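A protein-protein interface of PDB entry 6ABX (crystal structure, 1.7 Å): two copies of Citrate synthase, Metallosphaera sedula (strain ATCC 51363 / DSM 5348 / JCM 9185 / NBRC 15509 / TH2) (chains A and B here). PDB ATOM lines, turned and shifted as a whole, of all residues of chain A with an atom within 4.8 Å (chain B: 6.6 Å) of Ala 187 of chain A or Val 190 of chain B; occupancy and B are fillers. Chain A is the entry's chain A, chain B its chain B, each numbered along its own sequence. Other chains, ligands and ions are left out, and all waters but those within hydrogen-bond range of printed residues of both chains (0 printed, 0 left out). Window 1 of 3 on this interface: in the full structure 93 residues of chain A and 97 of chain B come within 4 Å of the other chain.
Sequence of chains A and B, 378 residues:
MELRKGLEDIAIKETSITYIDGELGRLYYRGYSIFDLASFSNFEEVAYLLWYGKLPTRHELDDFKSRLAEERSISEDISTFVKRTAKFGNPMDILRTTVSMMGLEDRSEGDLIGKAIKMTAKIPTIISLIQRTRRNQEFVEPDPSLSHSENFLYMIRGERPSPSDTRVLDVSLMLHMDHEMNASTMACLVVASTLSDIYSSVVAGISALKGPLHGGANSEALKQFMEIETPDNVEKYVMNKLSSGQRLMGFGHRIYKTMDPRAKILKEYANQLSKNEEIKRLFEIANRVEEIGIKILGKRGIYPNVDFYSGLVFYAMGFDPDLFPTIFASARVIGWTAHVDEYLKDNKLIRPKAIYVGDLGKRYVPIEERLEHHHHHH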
ATOM      1  N   ALA A 183      -2.728  31.904 -16.070  1.00  0.00           N
ATOM      2  CA  ALA A 183      -1.510  31.157 -15.710  1.00  0.00           C
ATOM      3  C   ALA A 183      -1.830  29.840 -14.997  1.00  0.00           C
ATOM      4  O   ALA A 183      -1.138  28.865 -15.203  1.00  0.00           O
ATOM      5  CB  ALA A 183      -0.622  32.002 -14.843  1.00  0.00           C
ATOM      6  N   SER A 184      -2.794  29.813 -14.069  1.00  0.00           N
ATOM      7  CA  SER A 184      -3.108  28.582 -13.356  1.00  0.00           C
ATOM      8  C   SER A 184      -3.736  27.533 -14.286  1.00  0.00           C
ATOM      9  O   SER A 184      -3.372  26.346 -14.184  1.00  0.00           O
ATOM     10  CB  SER A 184      -3.932  28.801 -12.103  1.00  0.00           C
ATOM     11  OG  SER A 184      -5.219  29.365 -12.386  1.00  0.00           O
ATOM     12  N   THR A 185      -4.657  27.944 -15.150  1.00  0.00           N
ATOM     13  CA  THR A 185      -5.218  27.006 -16.114  1.00  0.00           C
ATOM     14  C   THR A 185      -4.100  26.489 -17.031  1.00  0.00           C
ATOM     15  O   THR A 185      -4.080  25.272 -17.296  1.00  0.00           O
ATOM     16  CB  THR A 185      -6.366  27.665 -16.892  1.00  0.00           C
ATOM     17  OG1 THR A 185      -7.339  28.071 -15.922  1.00  0.00           O
ATOM     18  CG2 THR A 185      -6.939  26.764 -17.955  1.00  0.00           C
ATOM     19  N   MET A 186      -3.171  27.347 -17.422  1.00  0.00           N
ATOM     20  CA  MET A 186      -2.043  26.901 -18.244  1.00  0.00           C
ATOM     21  C   MET A 186      -1.209  25.848 -17.473  1.00  0.00           C
ATOM     22  O   MET A 186      -0.763  24.858 -18.030  1.00  0.00           O
ATOM     23  CB  MET A 186      -1.185  28.077 -18.711  1.00  0.00           C
ATOM     24  CG  MET A 186       0.033  27.704 -19.539  1.00  0.00           C
ATOM     25  SD  MET A 186      -0.492  26.889 -21.034  1.00  0.00           S
ATOM     26  CE  MET A 186       1.080  26.800 -21.893  1.00  0.00           C
ATOM     27  N   ALA A 187      -0.947  26.047 -16.189  1.00  0.00           N
ATOM     28  CA  ALA A 187      -0.158  25.067 -15.409  1.00  0.00           C
ATOM     29  C   ALA A 187      -0.844  23.706 -15.431  1.00  0.00           C
ATOM     30  O   ALA A 187      -0.212  22.680 -15.638  1.00  0.00           O
ATOM     31  CB  ALA A 187       0.035  25.558 -14.001  1.00  0.00           C
ATOM     32  N   CYS A 188      -2.181  23.721 -15.267  1.00  0.00           N
ATOM     33  CA  CYS A 188      -2.966  22.506 -15.245  1.00  0.00           C
ATOM     34  C   CYS A 188      -2.781  21.807 -16.594  1.00  0.00           C
ATOM     35  O   CYS A 188      -2.687  20.580 -16.617  1.00  0.00           O
ATOM     36  CB  CYS A 188      -4.441  22.742 -15.049  1.00  0.00           C
ATOM     37  SG  CYS A 188      -4.845  23.383 -13.396  1.00  0.00           S
ATOM     38  N   LEU A 189      -2.841  22.587 -17.676  1.00  0.00           N
ATOM     39  CA  LEU A 189      -2.817  22.024 -19.040  1.00  0.00           C
ATOM     40  C   LEU A 189      -1.419  21.489 -19.377  1.00  0.00           C
ATOM     41  O   LEU A 189      -1.344  20.450 -19.988  1.00  0.00           O
ATOM     42  CB  LEU A 189      -3.251  23.064 -20.057  1.00  0.00           C
ATOM     43  CG  LEU A 189      -4.739  23.360 -20.084  1.00  0.00           C
ATOM     44  CD1 LEU A 189      -5.005  24.636 -20.872  1.00  0.00           C
ATOM     45  CD2 LEU A 189      -5.490  22.203 -20.739  1.00  0.00           C
ATOM     46  N   VAL A 190      -0.351  22.168 -18.931  1.00  0.00           N
ATOM     47  CA  VAL A 190       1.005  21.648 -19.204  1.00  0.00           C
ATOM     48  C   VAL A 190       1.133  20.261 -18.582  1.00  0.00           C
ATOM     49  O   VAL A 190       1.583  19.305 -19.229  1.00  0.00           O
ATOM     50  CB  VAL A 190       2.098  22.583 -18.717  1.00  0.00           C
ATOM     51  CG1 VAL A 190       3.461  21.942 -18.880  1.00  0.00           C
ATOM     52  CG2 VAL A 190       2.045  23.884 -19.506  1.00  0.00           C
ATOM     53  N   VAL A 191       0.704  20.140 -17.329  1.00  0.00           N
ATOM     54  CA  VAL A 191       0.779  18.842 -16.626  1.00  0.00           C
ATOM     55  C   VAL A 191      -0.092  17.810 -17.333  1.00  0.00           C
ATOM     56  O   VAL A 191       0.320  16.665 -17.536  1.00  0.00           O
ATOM     57  CB  VAL A 191       0.370  19.022 -15.157  1.00  0.00           C
ATOM     58  CG1 VAL A 191       0.152  17.725 -14.429  1.00  0.00           C
ATOM     59  CG2 VAL A 191       1.407  19.861 -14.419  1.00  0.00           C
ATOM     60  N   ALA A 204      -0.778  21.502  -9.685  1.00  0.00           N
ATOM     61  CA  ALA A 204      -0.043  22.534 -10.369  1.00  0.00           C
ATOM     62  C   ALA A 204      -0.856  23.817 -10.485  1.00  0.00           C
ATOM     63  O   ALA A 204      -0.294  24.895 -10.328  1.00  0.00           O
ATOM     64  CB  ALA A 204       0.396  22.058 -11.718  1.00  0.00           C
ATOM     65  N   GLY A 205      -2.179  23.716 -10.742  1.00  0.00           N
ATOM     66  CA  GLY A 205      -3.061  24.896 -10.727  1.00  0.00           C
ATOM     67  C   GLY A 205      -2.966  25.703  -9.424  1.00  0.00           C
ATOM     68  O   GLY A 205      -2.761  26.910  -9.428  1.00  0.00           O
ATOM     69  N   ALA A 208       0.387  27.541  -9.018  1.00  0.00           N
ATOM     70  CA  ALA A 208       0.415  28.785  -9.814  1.00  0.00           C
ATOM     71  C   ALA A 208      -0.462  29.880  -9.192  1.00  0.00           C
ATOM     72  O   ALA A 208      -0.092  31.047  -9.107  1.00  0.00           O
ATOM     73  CB  ALA A 208      -0.029  28.517 -11.240  1.00  0.00           C
ATOM     74  N   THR B 185       9.855  21.340 -17.106  1.00  0.00           N
ATOM     75  CA  THR B 185      10.482  22.641 -16.900  1.00  0.00           C
ATOM     76  C   THR B 185       9.463  23.749 -17.197  1.00  0.00           C
ATOM     77  O   THR B 185       9.415  24.748 -16.459  1.00  0.00           O
ATOM     78  CB  THR B 185      11.764  22.823 -17.713  1.00  0.00           C
ATOM     79  OG1 THR B 185      12.638  21.781 -17.251  1.00  0.00           O
ATOM     80  CG2 THR B 185      12.409  24.179 -17.463  1.00  0.00           C
ATOM     81  N   MET B 186       8.650  23.557 -18.215  1.00  0.00           N
ATOM     82  CA  MET B 186       7.616  24.607 -18.556  1.00  0.00           C
ATOM     83  C   MET B 186       6.601  24.734 -17.410  1.00  0.00           C
ATOM     84  O   MET B 186       6.270  25.829 -16.984  1.00  0.00           O
ATOM     85  CB  MET B 186       6.917  24.241 -19.857  1.00  0.00           C
ATOM     86  CG  MET B 186       5.852  25.219 -20.321  1.00  0.00           C
ATOM     87  SD  MET B 186       6.509  26.863 -20.582  1.00  0.00           S
ATOM     88  CE  MET B 186       4.988  27.660 -21.118  1.00  0.00           C
ATOM     89  N   ALA B 187       6.156  23.613 -16.844  1.00  0.00           N
ATOM     90  CA  ALA B 187       5.265  23.651 -15.680  1.00  0.00           C
ATOM     91  C   ALA B 187       5.888  24.489 -14.561  1.00  0.00           C
ATOM     92  O   ALA B 187       5.199  25.318 -13.964  1.00  0.00           O
ATOM     93  CB  ALA B 187       4.900  22.258 -15.202  1.00  0.00           C
ATOM     94  N   CYS B 188       7.146  24.205 -14.219  1.00  0.00           N
ATOM     95  CA  CYS B 188       7.901  24.928 -13.168  1.00  0.00           C
ATOM     96  C   CYS B 188       7.882  26.427 -13.491  1.00  0.00           C
ATOM     97  O   CYS B 188       7.750  27.232 -12.612  1.00  0.00           O
ATOM     98  CB  CYS B 188       9.358  24.464 -13.048  1.00  0.00           C
ATOM     99  SG  CYS B 188       9.539  22.754 -12.463  1.00  0.00           S
ATOM    100  N   LEU B 189       8.146  26.782 -14.725  1.00  0.00           N
ATOM    101  CA  LEU B 189       8.263  28.193 -15.140  1.00  0.00           C
ATOM    102  C   LEU B 189       6.912  28.904 -15.099  1.00  0.00           C
ATOM    103  O   LEU B 189       6.881  30.068 -14.689  1.00  0.00           O
ATOM    104  CB  LEU B 189       8.874  28.330 -16.536  1.00  0.00           C
ATOM    105  CG  LEU B 189      10.359  28.046 -16.588  1.00  0.00           C
ATOM    106  CD1 LEU B 189      10.821  27.983 -18.039  1.00  0.00           C
ATOM    107  CD2 LEU B 189      11.150  29.109 -15.821  1.00  0.00           C
ATOM    108  N   VAL B 190       5.836  28.217 -15.530  1.00  0.00           N
ATOM    109  CA  VAL B 190       4.492  28.848 -15.478  1.00  0.00           C
ATOM    110  C   VAL B 190       4.201  29.238 -14.024  1.00  0.00           C
ATOM    111  O   VAL B 190       3.796  30.357 -13.714  1.00  0.00           O
ATOM    112  CB  VAL B 190       3.403  27.960 -16.090  1.00  0.00           C
ATOM    113  CG1 VAL B 190       1.993  28.504 -15.859  1.00  0.00           C
ATOM    114  CG2 VAL B 190       3.667  27.723 -17.572  1.00  0.00           C
ATOM    115  N   VAL B 191       4.404  28.283 -13.125  1.00  0.00           N
ATOM    116  CA  VAL B 191       4.215  28.541 -11.701  1.00  0.00           C
ATOM    117  C   VAL B 191       5.144  29.657 -11.195  1.00  0.00           C
ATOM    118  O   VAL B 191       4.702  30.546 -10.465  1.00  0.00           O
ATOM    119  CB  VAL B 191       4.427  27.259 -10.889  1.00  0.00           C
ATOM    120  CG1 VAL B 191       4.475  27.524  -9.388  1.00  0.00           C
ATOM    121  CG2 VAL B 191       3.358  26.244 -11.229  1.00  0.00           C
ATOM    122  N   ALA B 192       6.439  29.604 -11.543  1.00  0.00           N
ATOM    123  CA  ALA B 192       7.360  30.642 -11.073  1.00  0.00           C
ATOM    124  C   ALA B 192       6.962  32.038 -11.557  1.00  0.00           C
ATOM    125  O   ALA B 192       7.214  33.002 -10.835  1.00  0.00           O
ATOM    126  CB  ALA B 192       8.767  30.350 -11.519  1.00  0.00           C
ATOM    127  N   SER B 193       6.358  32.108 -12.742  1.00  0.00           N
ATOM    128  CA  SER B 193       6.068  33.354 -13.447  1.00  0.00           C
ATOM    129  C   SER B 193       4.998  34.163 -12.703  1.00  0.00           C
ATOM    130  O   SER B 193       4.878  35.370 -12.885  1.00  0.00           O
ATOM    131  CB  SER B 193       5.684  33.094 -14.891  1.00  0.00           C
ATOM    132  OG  SER B 193       4.305  32.729 -15.030  1.00  0.00           O
ATOM    133  N   THR B 194       4.252  33.507 -11.813  1.00  0.00           N
ATOM    134  CA  THR B 194       3.244  34.158 -10.953  1.00  0.00           C
ATOM    135  C   THR B 194       3.863  34.715  -9.660  1.00  0.00           C
ATOM    136  O   THR B 194       3.144  35.265  -8.855  1.00  0.00           O
ATOM    137  CB  THR B 194       2.100  33.206 -10.563  1.00  0.00           C
ATOM    138  OG1 THR B 194       2.616  32.201  -9.678  1.00  0.00           O
ATOM    139  CG2 THR B 194       1.413  32.548 -11.743  1.00  0.00           C
ATOM    140  N   LEU B 195       5.157  34.470  -9.455  1.00  0.00           N
ATOM    141  CA  LEU B 195       5.940  34.760  -8.277  1.00  0.00           C
ATOM    142  C   LEU B 195       5.522  33.821  -7.126  1.00  0.00           C
ATOM    143  O   LEU B 195       5.744  34.098  -5.953  1.00  0.00           O
ATOM    144  CB  LEU B 195       5.900  36.256  -7.928  1.00  0.00           C
ATOM    145  CG  LEU B 195       6.452  37.178  -9.015  1.00  0.00           C
ATOM    146  CD1 LEU B 195       6.395  38.632  -8.569  1.00  0.00           C
ATOM    147  CD2 LEU B 195       7.863  36.814  -9.425  1.00  0.00           C
ATOM    148  N   SER B 201       6.914  25.560  -7.588  1.00  0.00           N
ATOM    149  CA  SER B 201       7.463  25.268  -8.934  1.00  0.00           C
ATOM    150  C   SER B 201       7.840  23.788  -9.070  1.00  0.00           C
ATOM    151  O   SER B 201       7.447  23.099 -10.032  1.00  0.00           O
ATOM    152  CB  SER B 201       8.582  26.165  -9.370  1.00  0.00           C
ATOM    153  OG  SER B 201       8.170  27.518  -9.361  1.00  0.00           O
ATOM    154  N   ALA B 204       5.038  21.351  -9.207  1.00  0.00           N
ATOM    155  CA  ALA B 204       4.424  21.311 -10.554  1.00  0.00           C
ATOM    156  C   ALA B 204       5.313  20.540 -11.544  1.00  0.00           C
ATOM    157  O   ALA B 204       4.851  19.784 -12.364  1.00  0.00           O
ATOM    158  CB  ALA B 204       4.149  22.732 -11.051  1.00  0.00           C
ATOM    159  N   LEU B 349       4.841  37.210 -16.409  1.00  0.00           N
ATOM    160  CA  LEU B 349       3.753  36.310 -16.232  1.00  0.00           C
ATOM    161  C   LEU B 349       3.516  35.548 -17.529  1.00  0.00           C
ATOM    162  O   LEU B 349       3.448  36.150 -18.600  1.00  0.00           O
ATOM    163  CB  LEU B 349       2.481  37.080 -15.832  1.00  0.00           C
ATOM    164  CG  LEU B 349       1.257  36.217 -15.562  1.00  0.00           C
ATOM    165  CD1 LEU B 349       1.417  35.385 -14.304  1.00  0.00           C
ATOM    166  CD2 LEU B 349      -0.017  37.072 -15.443  1.00  0.00           C
ATOM    167  N   ILE B 350       3.336  34.227 -17.403  1.00  0.00           N
ATOM    168  CA  ILE B 350       2.999  33.414 -18.544  1.00  0.00           C
ATOM    169  C   ILE B 350       1.488  33.268 -18.609  1.00  0.00           C
ATOM    170  O   ILE B 350       0.877  32.589 -17.760  1.00  0.00           O
ATOM    171  CB  ILE B 350       3.753  32.069 -18.520  1.00  0.00           C
ATOM    172  CG1 ILE B 350       5.256  32.310 -18.644  1.00  0.00           C
ATOM    173  CG2 ILE B 350       3.212  31.163 -19.618  1.00  0.00           C
ATOM    174  CD1 ILE B 350       6.090  31.044 -18.395  1.00  0.00           C
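Ala 183 of chain A touches Val 190 of chain B (O to CG1, 3.2 Å). Thr 194 of chain B touches Ala 183 of chain A. Leu 349 of chain B touches Ala 183 of chain A. O of Ile 350 of chain B touches CB of Ala 183 of chain A, at 3.3 Å. Ala 187 of chain A touches Val 190 of chain B. N of Ala 187 of chain B touches CG1 of Val 190 of chain A, 3.8 Å away. O of Ala 204 of chain A touches CG2 of Val 191 of chain B, 3.996 Å away. Ala 204 of chain A touches Ala 204 of chain B. CG2 of Val 191 of chain B touches N of Ala 208 of chain A (3.9 Å).
Leu 189 of chain A touches none of the printed residues of chain B. Printed residues of chain B within 4 Å of Val 190 of chain A: Ala 187. Printed residues of chain B within 4 Å of Ala 204 of chain A: Val 191 (3.996 Å) and Ala 204 (3.9 Å). Of the printed residues of chain A, Ala 187 of chain B touches Val 190 (3.8 Å). Val 190 of chain B touches just these residues of chain A: Ala 183 and Ala 187. Ala 192 of chain B touches none of the printed residues of chain A.
Ala 187 of chain A touches Val 190 of chain B, and with the chains exchanged Val 190 of chain A touches Ala 187 of chain B. Ala 204 of chain A touches Val 191 of chain B, but with the chains exchanged Val 191 of chain A does not touch Ala 204 of chain B (4.01 Å). Ala 204 of chain B touches its own counterpart, Ala 204 of chain A. Of the 10 pairs that touch across the chains among the printed residues, 3 have their exchanged pair printed and touching as well.
Hydrophobic or aromatic side chains of chain B within 4 Å of the printed part of chain A: Ala 187, Val 190, Val 191, Ala 204 and Leu 349. Among the printed residues, 10 pairs touch across the chains.
OG of Ser 193 of chain B sits at hydrogen-bond distance from O of Val 190 of chain B, at 2.8 Å. The backbone carbonyl oxygen of Val 191 of chain B lies within hydrogen-bond range of the side-chain hydroxyl of Thr 194 of chain B, at 2.8 Å. The side-chain hydroxyl of Ser 193 of chain B sits at hydrogen-bond distance from the backbone NH of Ile 350 of chain B (3.0 Å).
The side-chain hydroxyl (OG1) of Thr 194 of chain B lies within hydrogen-bond range of the backbone carbonyl oxygen (O) of Ala 208 of chain A.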
